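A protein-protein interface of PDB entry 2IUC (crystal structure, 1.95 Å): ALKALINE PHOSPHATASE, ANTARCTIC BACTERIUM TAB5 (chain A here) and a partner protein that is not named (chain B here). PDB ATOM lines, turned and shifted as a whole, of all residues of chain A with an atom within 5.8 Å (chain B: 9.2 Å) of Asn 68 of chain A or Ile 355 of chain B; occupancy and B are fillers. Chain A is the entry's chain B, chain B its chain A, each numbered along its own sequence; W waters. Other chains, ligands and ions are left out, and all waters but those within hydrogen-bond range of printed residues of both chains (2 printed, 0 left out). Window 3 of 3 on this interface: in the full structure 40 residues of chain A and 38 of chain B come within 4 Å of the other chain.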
ATOM      1  N   PHE A  66       2.303  21.462 -20.124  1.00  0.00           N
ATOM      2  CA  PHE A  66       3.789  21.304 -20.110  1.00  0.00           C
ATOM      3  C   PHE A  66       4.506  22.621 -19.880  1.00  0.00           C
ATOM      4  O   PHE A  66       4.150  23.674 -20.456  1.00  0.00           O
ATOM      5  CB  PHE A  66       4.354  20.669 -21.415  1.00  0.00           C
ATOM      6  CG  PHE A  66       3.955  19.263 -21.628  1.00  0.00           C
ATOM      7  CD1 PHE A  66       2.866  18.974 -22.474  1.00  0.00           C
ATOM      8  CD2 PHE A  66       4.617  18.213 -20.945  1.00  0.00           C
ATOM      9  CE1 PHE A  66       2.524  17.663 -22.727  1.00  0.00           C
ATOM     10  CE2 PHE A  66       4.303  16.881 -21.195  1.00  0.00           C
ATOM     11  CZ  PHE A  66       3.220  16.606 -21.999  1.00  0.00           C
ATOM     12  N   LYS A  67       5.520  22.526 -19.028  1.00  0.00           N
ATOM     13  CA  LYS A  67       6.419  23.609 -18.741  1.00  0.00           C
ATOM     14  C   LYS A  67       7.753  23.355 -19.471  1.00  0.00           C
ATOM     15  O   LYS A  67       8.267  24.250 -20.200  1.00  0.00           O
ATOM     16  CB  LYS A  67       6.730  23.710 -17.225  1.00  0.00           C
ATOM     17  CG  LYS A  67       5.544  24.165 -16.331  1.00  0.00           C
ATOM     18  CD  LYS A  67       4.703  25.220 -17.034  1.00  0.00           C
ATOM     19  CE  LYS A  67       3.359  25.496 -16.303  1.00  0.00           C
ATOM     20  NZ  LYS A  67       2.574  26.539 -17.087  1.00  0.00           N
ATOM     21  N   ASN A  68       8.329  22.175 -19.241  1.00  0.00           N
ATOM     22  CA  ASN A  68       9.608  21.833 -19.844  1.00  0.00           C
ATOM     23  C   ASN A  68       9.485  21.462 -21.300  1.00  0.00           C
ATOM     24  O   ASN A  68       8.826  20.497 -21.617  1.00  0.00           O
ATOM     25  CB  ASN A  68      10.283  20.729 -19.052  1.00  0.00           C
ATOM     26  CG  ASN A  68      10.582  21.144 -17.621  1.00  0.00           C
ATOM     27  OD1 ASN A  68      11.046  22.269 -17.329  1.00  0.00           O
ATOM     28  ND2 ASN A  68      10.352  20.238 -16.734  1.00  0.00           N
ATOM     29  N   ILE A  69      10.199  22.184 -22.180  1.00  0.00           N
ATOM     30  CA  ILE A  69      10.078  22.060 -23.620  1.00  0.00           C
ATOM     31  C   ILE A  69      11.483  22.070 -24.266  1.00  0.00           C
ATOM     32  O   ILE A  69      12.320  22.872 -23.876  1.00  0.00           O
ATOM     33  CB  ILE A  69       9.235  23.219 -24.189  1.00  0.00           C
ATOM     34  CG1 ILE A  69       7.778  23.048 -23.735  1.00  0.00           C
ATOM     35  CG2 ILE A  69       9.179  23.182 -25.728  1.00  0.00           C
ATOM     36  CD1 ILE A  69       6.894  24.293 -23.991  1.00  0.00           C
ATOM     37  N   GLY A  70      11.742  21.108 -25.163  1.00  0.00           N
ATOM     38  CA  GLY A  70      12.957  21.054 -25.946  1.00  0.00           C
ATOM     39  C   GLY A  70      12.708  20.989 -27.459  1.00  0.00           C
ATOM     40  O   GLY A  70      11.550  21.078 -27.913  1.00  0.00           O
ATOM     41  N   VAL A 344       9.746  18.938 -28.241  1.00  0.00           N
ATOM     42  CA  VAL A 344       9.611  17.836 -27.277  1.00  0.00           C
ATOM     43  C   VAL A 344       8.997  18.391 -25.990  1.00  0.00           C
ATOM     44  O   VAL A 344       9.498  19.378 -25.487  1.00  0.00           O
ATOM     45  CB  VAL A 344      11.039  17.400 -26.873  1.00  0.00           C
ATOM     46  CG1 VAL A 344      10.984  16.312 -25.728  1.00  0.00           C
ATOM     47  CG2 VAL A 344      11.817  16.922 -28.127  1.00  0.00           C
ATOM     48  N   PHE A 345       8.006  17.726 -25.413  1.00  0.00           N
ATOM     49  CA  PHE A 345       7.380  18.196 -24.183  1.00  0.00           C
ATOM     50  C   PHE A 345       7.674  17.132 -23.159  1.00  0.00           C
ATOM     51  O   PHE A 345       7.564  15.927 -23.507  1.00  0.00           O
ATOM     52  CB  PHE A 345       5.847  18.298 -24.351  1.00  0.00           C
ATOM     53  CG  PHE A 345       5.449  19.234 -25.469  1.00  0.00           C
ATOM     54  CD1 PHE A 345       5.337  20.597 -25.230  1.00  0.00           C
ATOM     55  CD2 PHE A 345       5.365  18.787 -26.780  1.00  0.00           C
ATOM     56  CE1 PHE A 345       4.962  21.498 -26.274  1.00  0.00           C
ATOM     57  CE2 PHE A 345       4.995  19.713 -27.826  1.00  0.00           C
ATOM     58  CZ  PHE A 345       4.807  21.061 -27.506  1.00  0.00           C
ATOM     59  N   ALA A 346       8.065  17.523 -21.956  1.00  0.00           N
ATOM     60  CA  ALA A 346       8.228  16.575 -20.801  1.00  0.00           C
ATOM     61  C   ALA A 346       7.656  17.058 -19.431  1.00  0.00           C
ATOM     62  O   ALA A 346       7.808  18.236 -19.051  1.00  0.00           O
ATOM     63  CB  ALA A 346       9.680  16.202 -20.629  1.00  0.00           C
ATOM     64  N   TYR A 347       7.057  16.139 -18.678  1.00  0.00           N
ATOM     65  CA  TYR A 347       6.401  16.472 -17.441  1.00  0.00           C
ATOM     66  C   TYR A 347       6.751  15.344 -16.494  1.00  0.00           C
ATOM     67  O   TYR A 347       6.668  14.207 -16.887  1.00  0.00           O
ATOM     68  CB  TYR A 347       4.863  16.474 -17.588  1.00  0.00           C
ATOM     69  CG  TYR A 347       4.221  16.651 -16.227  1.00  0.00           C
ATOM     70  CD1 TYR A 347       4.058  17.927 -15.691  1.00  0.00           C
ATOM     71  CD2 TYR A 347       3.879  15.525 -15.419  1.00  0.00           C
ATOM     72  CE1 TYR A 347       3.552  18.083 -14.395  1.00  0.00           C
ATOM     73  CE2 TYR A 347       3.399  15.675 -14.112  1.00  0.00           C
ATOM     74  CZ  TYR A 347       3.225  16.956 -13.602  1.00  0.00           C
ATOM     75  OH  TYR A 347       2.718  17.141 -12.296  1.00  0.00           O
ATOM     76  N   GLY A 348       7.102  15.627 -15.255  1.00  0.00           N
ATOM     77  CA  GLY A 348       7.250  14.551 -14.282  1.00  0.00           C
ATOM     78  C   GLY A 348       8.722  14.490 -13.855  1.00  0.00           C
ATOM     79  O   GLY A 348       9.527  15.254 -14.323  1.00  0.00           O
ATOM     80  N   SER A 351      12.090  15.502 -16.040  1.00  0.00           N
ATOM     81  CA  SER A 351      11.674  16.162 -17.291  1.00  0.00           C
ATOM     82  C   SER A 351      12.615  17.323 -17.703  1.00  0.00           C
ATOM     83  O   SER A 351      12.731  17.665 -18.908  1.00  0.00           O
ATOM     84  CB  SER A 351      10.187  16.629 -17.152  1.00  0.00           C
ATOM     85  OG  SER A 351      10.070  17.566 -16.062  1.00  0.00           O
ATOM     86  N   GLU A 352      13.321  17.910 -16.729  1.00  0.00           N
ATOM     87  CA  GLU A 352      14.244  19.031 -16.985  1.00  0.00           C
ATOM     88  C   GLU A 352      15.356  18.548 -17.927  1.00  0.00           C
ATOM     89  O   GLU A 352      15.929  19.399 -18.609  1.00  0.00           O
ATOM     90  CB  GLU A 352      14.944  19.580 -15.730  1.00  0.00           C
ATOM     91  CG  GLU A 352      14.071  20.302 -14.748  1.00  0.00           C
ATOM     92  CD  GLU A 352      13.104  19.382 -13.901  1.00  0.00           C
ATOM     93  OE1 GLU A 352      13.137  18.097 -13.877  1.00  0.00           O
ATOM     94  OE2 GLU A 352      12.254  20.035 -13.278  1.00  0.00           O
ATOM     95  N   ILE A 355      14.985  19.635 -22.015  1.00  0.00           N
ATOM     96  CA  ILE A 355      14.932  21.023 -22.491  1.00  0.00           C
ATOM     97  C   ILE A 355      16.101  21.260 -23.417  1.00  0.00           C
ATOM     98  O   ILE A 355      16.913  20.373 -23.610  1.00  0.00           O
ATOM     99  CB  ILE A 355      14.827  21.993 -21.324  1.00  0.00           C
ATOM    100  CG1 ILE A 355      16.137  22.017 -20.424  1.00  0.00           C
ATOM    101  CG2 ILE A 355      13.518  21.582 -20.468  1.00  0.00           C
ATOM    102  CD1 ILE A 355      16.127  23.097 -19.243  1.00  0.00           C
ATOM    103  N   LYS B  67      18.679  26.858 -23.165  1.00  0.00           N
ATOM    104  CA  LYS B  67      18.052  25.681 -22.563  1.00  0.00           C
ATOM    105  C   LYS B  67      16.547  25.986 -22.294  1.00  0.00           C
ATOM    106  O   LYS B  67      15.670  25.082 -22.515  1.00  0.00           O
ATOM    107  CB  LYS B  67      18.814  25.281 -21.272  1.00  0.00           C
ATOM    108  CG  LYS B  67      20.328  25.103 -21.505  1.00  0.00           C
ATOM    109  CD  LYS B  67      20.496  23.724 -22.267  1.00  0.00           C
ATOM    110  CE  LYS B  67      22.019  23.422 -22.713  1.00  0.00           C
ATOM    111  NZ  LYS B  67      22.156  22.488 -23.965  1.00  0.00           N
ATOM    112  N   ASN B  68      16.232  27.191 -21.780  1.00  0.00           N
ATOM    113  CA  ASN B  68      14.833  27.482 -21.390  1.00  0.00           C
ATOM    114  C   ASN B  68      14.094  27.907 -22.643  1.00  0.00           C
ATOM    115  O   ASN B  68      14.548  28.876 -23.290  1.00  0.00           O
ATOM    116  CB  ASN B  68      14.716  28.531 -20.291  1.00  0.00           C
ATOM    117  CG  ASN B  68      15.368  28.040 -18.999  1.00  0.00           C
ATOM    118  OD1 ASN B  68      15.097  26.916 -18.558  1.00  0.00           O
ATOM    119  ND2 ASN B  68      16.248  28.839 -18.437  1.00  0.00           N
ATOM    120  N   ILE B  69      13.016  27.198 -22.963  1.00  0.00           N
ATOM    121  CA  ILE B  69      12.245  27.407 -24.220  1.00  0.00           C
ATOM    122  C   ILE B  69      10.783  27.403 -23.852  1.00  0.00           C
ATOM    123  O   ILE B  69      10.333  26.577 -22.990  1.00  0.00           O
ATOM    124  CB  ILE B  69      12.603  26.289 -25.335  1.00  0.00           C
ATOM    125  CG1 ILE B  69      14.067  26.428 -25.873  1.00  0.00           C
ATOM    126  CG2 ILE B  69      11.633  26.307 -26.566  1.00  0.00           C
ATOM    127  CD1 ILE B  69      14.649  25.108 -26.425  1.00  0.00           C
ATOM    128  N   GLY B  70      10.037  28.329 -24.463  1.00  0.00           N
ATOM    129  CA  GLY B  70       8.586  28.340 -24.265  1.00  0.00           C
ATOM    130  C   GLY B  70       7.923  28.537 -25.589  1.00  0.00           C
ATOM    131  O   GLY B  70       8.603  28.579 -26.628  1.00  0.00           O
ATOM    132  N   LEU B  71       6.615  28.711 -25.553  1.00  0.00           N
ATOM    133  CA  LEU B  71       5.848  28.826 -26.804  1.00  0.00           C
ATOM    134  C   LEU B  71       4.761  29.876 -26.576  1.00  0.00           C
ATOM    135  O   LEU B  71       4.100  29.895 -25.489  1.00  0.00           O
ATOM    136  CB  LEU B  71       5.194  27.474 -27.207  1.00  0.00           C
ATOM    137  CG  LEU B  71       5.981  26.252 -27.617  1.00  0.00           C
ATOM    138  CD1 LEU B  71       5.011  24.994 -27.636  1.00  0.00           C
ATOM    139  CD2 LEU B  71       6.684  26.520 -28.992  1.00  0.00           C
ATOM    140  N   ILE B  72       4.582  30.768 -27.577  1.00  0.00           N
ATOM    141  CA  ILE B  72       3.503  31.771 -27.472  1.00  0.00           C
ATOM    142  C   ILE B  72       2.401  31.634 -28.515  1.00  0.00           C
ATOM    143  O   ILE B  72       2.666  31.353 -29.664  1.00  0.00           O
ATOM    144  CB  ILE B  72       4.071  33.246 -27.552  1.00  0.00           C
ATOM    145  CG1 ILE B  72       4.988  33.464 -28.798  1.00  0.00           C
ATOM    146  CG2 ILE B  72       4.726  33.647 -26.232  1.00  0.00           C
ATOM    147  CD1 ILE B  72       5.436  35.029 -28.966  1.00  0.00           C
ATOM    148  N   VAL B 344       9.929  30.704 -27.905  1.00  0.00           N
ATOM    149  CA  VAL B 344      10.484  31.777 -27.196  1.00  0.00           C
ATOM    150  C   VAL B 344      11.770  31.128 -26.606  1.00  0.00           C
ATOM    151  O   VAL B 344      11.708  30.062 -26.012  1.00  0.00           O
ATOM    152  CB  VAL B 344       9.580  32.199 -25.990  1.00  0.00           C
ATOM    153  CG1 VAL B 344      10.282  33.321 -25.101  1.00  0.00           C
ATOM    154  CG2 VAL B 344       8.210  32.683 -26.479  1.00  0.00           C
ATOM    155  N   PHE B 345      12.902  31.797 -26.714  1.00  0.00           N
ATOM    156  CA  PHE B 345      14.162  31.315 -26.075  1.00  0.00           C
ATOM    157  C   PHE B 345      14.602  32.313 -25.009  1.00  0.00           C
ATOM    158  O   PHE B 345      14.543  33.544 -25.264  1.00  0.00           O
ATOM    159  CB  PHE B 345      15.265  31.196 -27.202  1.00  0.00           C
ATOM    160  CG  PHE B 345      14.840  30.321 -28.343  1.00  0.00           C
ATOM    161  CD1 PHE B 345      15.150  28.947 -28.353  1.00  0.00           C
ATOM    162  CD2 PHE B 345      14.085  30.853 -29.388  1.00  0.00           C
ATOM    163  CE1 PHE B 345      14.728  28.152 -29.393  1.00  0.00           C
ATOM    164  CE2 PHE B 345      13.650  30.072 -30.425  1.00  0.00           C
ATOM    165  CZ  PHE B 345      13.944  28.737 -30.446  1.00  0.00           C
ATOM    166  N   ALA B 346      15.101  31.845 -23.823  1.00  0.00           N
ATOM    167  CA  ALA B 346      15.479  32.763 -22.793  1.00  0.00           C
ATOM    168  C   ALA B 346      16.774  32.273 -22.111  1.00  0.00           C
ATOM    169  O   ALA B 346      16.914  31.098 -21.807  1.00  0.00           O
ATOM    170  CB  ALA B 346      14.290  32.952 -21.671  1.00  0.00           C
ATOM    171  N   TYR B 347      17.696  33.183 -21.907  1.00  0.00           N
ATOM    172  CA  TYR B 347      18.949  32.870 -21.256  1.00  0.00           C
ATOM    173  C   TYR B 347      19.172  33.986 -20.263  1.00  0.00           C
ATOM    174  O   TYR B 347      18.904  35.177 -20.612  1.00  0.00           O
ATOM    175  CB  TYR B 347      20.090  32.825 -22.325  1.00  0.00           C
ATOM    176  CG  TYR B 347      21.414  32.581 -21.627  1.00  0.00           C
ATOM    177  CD1 TYR B 347      21.831  31.297 -21.317  1.00  0.00           C
ATOM    178  CD2 TYR B 347      22.192  33.662 -21.193  1.00  0.00           C
ATOM    179  CE1 TYR B 347      23.054  31.110 -20.591  1.00  0.00           C
ATOM    180  CE2 TYR B 347      23.371  33.469 -20.471  1.00  0.00           C
ATOM    181  CZ  TYR B 347      23.792  32.211 -20.198  1.00  0.00           C
ATOM    182  OH  TYR B 347      24.998  32.043 -19.506  1.00  0.00           O
ATOM    183  N   GLY B 350      16.249  34.912 -14.348  1.00  0.00           N
ATOM    184  CA  GLY B 350      14.830  34.846 -14.653  1.00  0.00           C
ATOM    185  C   GLY B 350      14.348  34.106 -15.904  1.00  0.00           C
ATOM    186  O   GLY B 350      13.153  34.151 -16.192  1.00  0.00           O
ATOM    187  N   SER B 351      15.250  33.489 -16.678  1.00  0.00           N
ATOM    188  CA  SER B 351      14.921  32.827 -17.991  1.00  0.00           C
ATOM    189  C   SER B 351      13.897  31.674 -17.838  1.00  0.00           C
ATOM    190  O   SER B 351      13.070  31.445 -18.747  1.00  0.00           O
ATOM    191  CB  SER B 351      16.145  32.268 -18.711  1.00  0.00           C
ATOM    192  OG  SER B 351      16.861  31.345 -17.901  1.00  0.00           O
ATOM    193  N   GLU B 352      13.909  31.027 -16.657  1.00  0.00           N
ATOM    194  CA  GLU B 352      12.877  30.000 -16.309  1.00  0.00           C
ATOM    195  C   GLU B 352      11.438  30.535 -16.349  1.00  0.00           C
ATOM    196  O   GLU B 352      10.512  29.752 -16.458  1.00  0.00           O
ATOM    197  CB  GLU B 352      13.074  29.517 -14.866  1.00  0.00           C
ATOM    198  CG  GLU B 352      14.278  28.628 -14.672  1.00  0.00           C
ATOM    199  CD  GLU B 352      15.586  29.405 -14.344  1.00  0.00           C
ATOM    200  OE1 GLU B 352      15.583  30.707 -14.247  1.00  0.00           O
ATOM    201  OE2 GLU B 352      16.608  28.647 -14.182  1.00  0.00           O
ATOM    202  N   GLU B 353      11.224  31.840 -16.139  1.00  0.00           N
ATOM    203  CA  GLU B 353       9.838  32.422 -16.197  1.00  0.00           C
ATOM    204  C   GLU B 353       9.190  32.306 -17.601  1.00  0.00           C
ATOM    205  O   GLU B 353       7.950  32.355 -17.731  1.00  0.00           O
ATOM    206  CB  GLU B 353       9.897  33.920 -15.786  1.00  0.00           C
ATOM    207  CG  GLU B 353       8.578  34.479 -15.293  1.00  0.00           C
ATOM    208  CD  GLU B 353       8.059  33.692 -14.073  1.00  0.00           C
ATOM    209  OE1 GLU B 353       8.855  33.276 -13.162  1.00  0.00           O
ATOM    210  OE2 GLU B 353       6.826  33.483 -14.053  1.00  0.00           O
ATOM    211  N   PHE B 354      10.028  32.115 -18.644  1.00  0.00           N
ATOM    212  CA  PHE B 354       9.566  32.089 -20.018  1.00  0.00           C
ATOM    213  C   PHE B 354       9.284  30.694 -20.672  1.00  0.00           C
ATOM    214  O   PHE B 354       9.055  30.631 -21.876  1.00  0.00           O
ATOM    215  CB  PHE B 354      10.624  32.880 -20.844  1.00  0.00           C
ATOM    216  CG  PHE B 354      10.719  34.332 -20.396  1.00  0.00           C
ATOM    217  CD1 PHE B 354       9.981  35.323 -21.021  1.00  0.00           C
ATOM    218  CD2 PHE B 354      11.512  34.689 -19.337  1.00  0.00           C
ATOM    219  CE1 PHE B 354      10.026  36.682 -20.616  1.00  0.00           C
ATOM    220  CE2 PHE B 354      11.574  36.060 -18.915  1.00  0.00           C
ATOM    221  CZ  PHE B 354      10.797  37.018 -19.579  1.00  0.00           C
ATOM    222  N   ILE B 355       9.266  29.617 -19.886  1.00  0.00           N
ATOM    223  CA  ILE B 355       8.982  28.266 -20.380  1.00  0.00           C
ATOM    224  C   ILE B 355       7.475  28.017 -20.350  1.00  0.00           C
ATOM    225  O   ILE B 355       6.727  28.882 -19.929  1.00  0.00           O
ATOM    226  CB  ILE B 355       9.778  27.224 -19.555  1.00  0.00           C
ATOM    227  CG1 ILE B 355       9.215  27.073 -18.123  1.00  0.00           C
ATOM    228  CG2 ILE B 355      11.284  27.616 -19.518  1.00  0.00           C
ATOM    229  CD1 ILE B 355       9.853  26.054 -17.320  1.00  0.00           C
ATOM    230  N   GLY B 356       7.009  26.928 -20.910  1.00  0.00           N
ATOM    231  CA  GLY B 356       5.632  26.694 -20.949  1.00  0.00           C
ATOM    232  C   GLY B 356       4.976  27.372 -22.138  1.00  0.00           C
ATOM    233  O   GLY B 356       5.666  27.866 -23.047  1.00  0.00           O
ATOM    234  N   ILE B 357       3.647  27.298 -22.151  1.00  0.00           N
ATOM    235  CA  ILE B 357       2.817  27.836 -23.281  1.00  0.00           C
ATOM    236  C   ILE B 357       1.914  28.978 -22.766  1.00  0.00           C
ATOM    237  O   ILE B 357       1.239  28.817 -21.770  1.00  0.00           O
ATOM    238  CB  ILE B 357       1.971  26.722 -23.975  1.00  0.00           C
ATOM    239  CG1 ILE B 357       2.907  25.597 -24.445  1.00  0.00           C
ATOM    240  CG2 ILE B 357       1.169  27.314 -25.190  1.00  0.00           C
ATOM    241  CD1 ILE B 357       2.229  24.382 -25.115  1.00  0.00           C
ATOM    242  N   TYR B 358       2.015  30.171 -23.380  1.00  0.00           N
ATOM    243  CA  TYR B 358       1.311  31.353 -22.870  1.00  0.00           C
ATOM    244  C   TYR B 358       0.955  32.239 -24.045  1.00  0.00           C
ATOM    245  O   TYR B 358       1.483  32.028 -25.153  1.00  0.00           O
ATOM    246  CB  TYR B 358       2.100  32.155 -21.810  1.00  0.00           C
ATOM    247  CG  TYR B 358       3.578  32.357 -22.099  1.00  0.00           C
ATOM    248  CD1 TYR B 358       4.030  33.525 -22.725  1.00  0.00           C
ATOM    249  CD2 TYR B 358       4.519  31.372 -21.721  1.00  0.00           C
ATOM    250  CE1 TYR B 358       5.418  33.735 -22.985  1.00  0.00           C
ATOM    251  CE2 TYR B 358       5.871  31.543 -21.964  1.00  0.00           C
ATOM    252  CZ  TYR B 358       6.324  32.733 -22.611  1.00  0.00           C
ATOM    253  OH  TYR B 358       7.686  32.926 -22.843  1.00  0.00           O
ATOM    254  N   GLU B 359       0.088  33.225 -23.817  1.00  0.00           N
ATOM    255  CA  GLU B 359      -0.268  34.183 -24.880  1.00  0.00           C
ATOM    256  C   GLU B 359       0.917  35.186 -25.095  1.00  0.00           C
ATOM    257  O   GLU B 359       1.651  35.510 -24.144  1.00  0.00           O
ATOM    258  CB  GLU B 359      -1.486  34.985 -24.419  1.00  0.00           C
ATOM    259  CG  GLU B 359      -2.791  34.204 -24.214  1.00  0.00           C
ATOM    260  CD  GLU B 359      -3.411  33.763 -25.488  1.00  0.00           C
ATOM    261  OE1 GLU B 359      -2.998  34.302 -26.556  1.00  0.00           O
ATOM    262  OE2 GLU B 359      -4.245  32.806 -25.449  1.00  0.00           O
ATOM    263  N   GLU B 362       1.965  38.071 -22.692  1.00  0.00           N
ATOM    264  CA  GLU B 362       2.489  37.779 -21.393  1.00  0.00           C
ATOM    265  C   GLU B 362       3.996  37.929 -21.403  1.00  0.00           C
ATOM    266  O   GLU B 362       4.604  37.892 -20.345  1.00  0.00           O
ATOM    267  CB  GLU B 362       2.075  36.365 -20.943  1.00  0.00           C
ATOM    268  CG  GLU B 362       0.582  36.173 -20.801  1.00  0.00           C
ATOM    269  CD  GLU B 362       0.045  36.960 -19.620  1.00  0.00           C
ATOM    270  OE1 GLU B 362       0.768  37.128 -18.606  1.00  0.00           O
ATOM    271  OE2 GLU B 362      -1.123  37.380 -19.662  1.00  0.00           O
ATOM    272  N   ILE B 363       4.617  38.109 -22.579  1.00  0.00           N
ATOM    273  CA  ILE B 363       6.037  38.409 -22.613  1.00  0.00           C
ATOM    274  C   ILE B 363       6.344  39.685 -21.778  1.00  0.00           C
ATOM    275  O   ILE B 363       7.279  39.708 -20.944  1.00  0.00           O
ATOM    276  CB  ILE B 363       6.532  38.514 -24.118  1.00  0.00           C
ATOM    277  CG1 ILE B 363       6.578  37.127 -24.806  1.00  0.00           C
ATOM    278  CG2 ILE B 363       7.854  39.285 -24.246  1.00  0.00           C
ATOM    279  CD1 ILE B 363       7.794  36.228 -24.293  1.00  0.00           C
ATOM    280  N   LYS B 366       5.972  39.037 -17.996  1.00  0.00           N
ATOM    281  CA  LYS B 366       7.074  38.219 -17.531  1.00  0.00           C
ATOM    282  C   LYS B 366       8.382  39.023 -17.362  1.00  0.00           C
ATOM    283  O   LYS B 366       9.110  38.858 -16.391  1.00  0.00           O
ATOM    284  CB  LYS B 366       7.243  36.983 -18.485  1.00  0.00           C
ATOM    285  CG  LYS B 366       6.088  35.979 -18.354  1.00  0.00           C
ATOM    286  CD  LYS B 366       6.212  34.923 -19.433  1.00  0.00           C
ATOM    287  CE  LYS B 366       5.241  33.786 -19.234  1.00  0.00           C
ATOM    288  NZ  LYS B 366       5.413  33.012 -17.967  1.00  0.00           N
HETATM  289  O   HOH W   1       2.310  25.734 -20.197  1.00  0.00           O
HETATM  290  O   HOH W   2      11.836  24.768 -21.717  1.00  0.00           O
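The backbone NH of Gly 356 of chain B is in hydrogen-bond range of the backbone carbonyl oxygen of Lys 67 of chain A (3.0 Å).
O of Leu 71 of chain B lies within hydrogen-bond range of N of Tyr 358 of chain B, 3.0 Å away. N of Ala 346 of chain A lies within hydrogen-bond range of O of Asn 68 of chain A (3.1 Å). The backbone NH of Leu 71 of chain B sits at hydrogen-bond distance from the backbone carbonyl oxygen of Gly 356 of chain B, 2.8 Å away. The side-chain hydroxyl (OG) of Ser 351 of chain A sits at hydrogen-bond distance from the side-chain amide nitrogen (ND2) of Asn 68 of chain A, at 2.8 Å.
O of Phe 66 of chain A touches CA of Gly 356 of chain B (3.4 Å). Lys 67 of chain A touches Ile 355 of chain B (O to CB, 3.4 Å). CD1 of Ile 355 of chain B touches OD1 of Asn 68 of chain A, 3.97 Å away. Ile 69 of chain A touches Ile 69 of chain B. Gly 356 of chain B touches Ile 69 of chain A. CD1 of Leu 71 of chain B touches CE1 of Phe 345 of chain A (3.8 Å). Ile 355 of chain A touches Lys 67 of chain B (CB to O, 3.4 Å).
Asn 68 of chain A touches just one residue of chain B: Ile 355 (3.97 Å). Ile 69 of chain A touches just these residues of chain B: Ile 69 (3.7 Å) and Gly 356 (3.9 Å). No residue of chain B comes within 4 Å of Ala 346 of chain A. No residue of chain B comes within 4 Å of Ser 351 of chain A. Of the printed residues of chain B, Ile 355 of chain A touches Lys 67. Of the printed residues of chain A, Ile 69 of chain B touches Ile 69. Of chain A, only Lys 67 (3.4 Å) and Asn 68 (3.97 Å) come within 4 Å of Ile 355 of chain B. The nearest residue of chain B that does not touch Asn 68 of chain A is Gly 356 of chain B (5.2 Å).
Hydrophobic or aromatic side chains of chain B that line the printed part of chain A: Ile 69, Leu 71 and Ile 355. Of the 13 printed residues of chain A, 6 touch a printed residue of chain B. Among the printed residues, 8 pairs touch across the chains. Among the printed residues, no Asp or Glu carboxylate lies within 4 Å of a Lys or Arg side-chain nitrogen of the other chain.
Water W2 bridges O of Ile 69 of chain B (2.7 Å) and O of Ile 69 of chain A (2.9 Å). Water W1 lies within hydrogen-bond range of O of Phe 66 of chain A (2.8 Å), N of Ile 357 of chain B (2.8 Å) and NZ of Lys 67 of chain A (3.2 Å).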
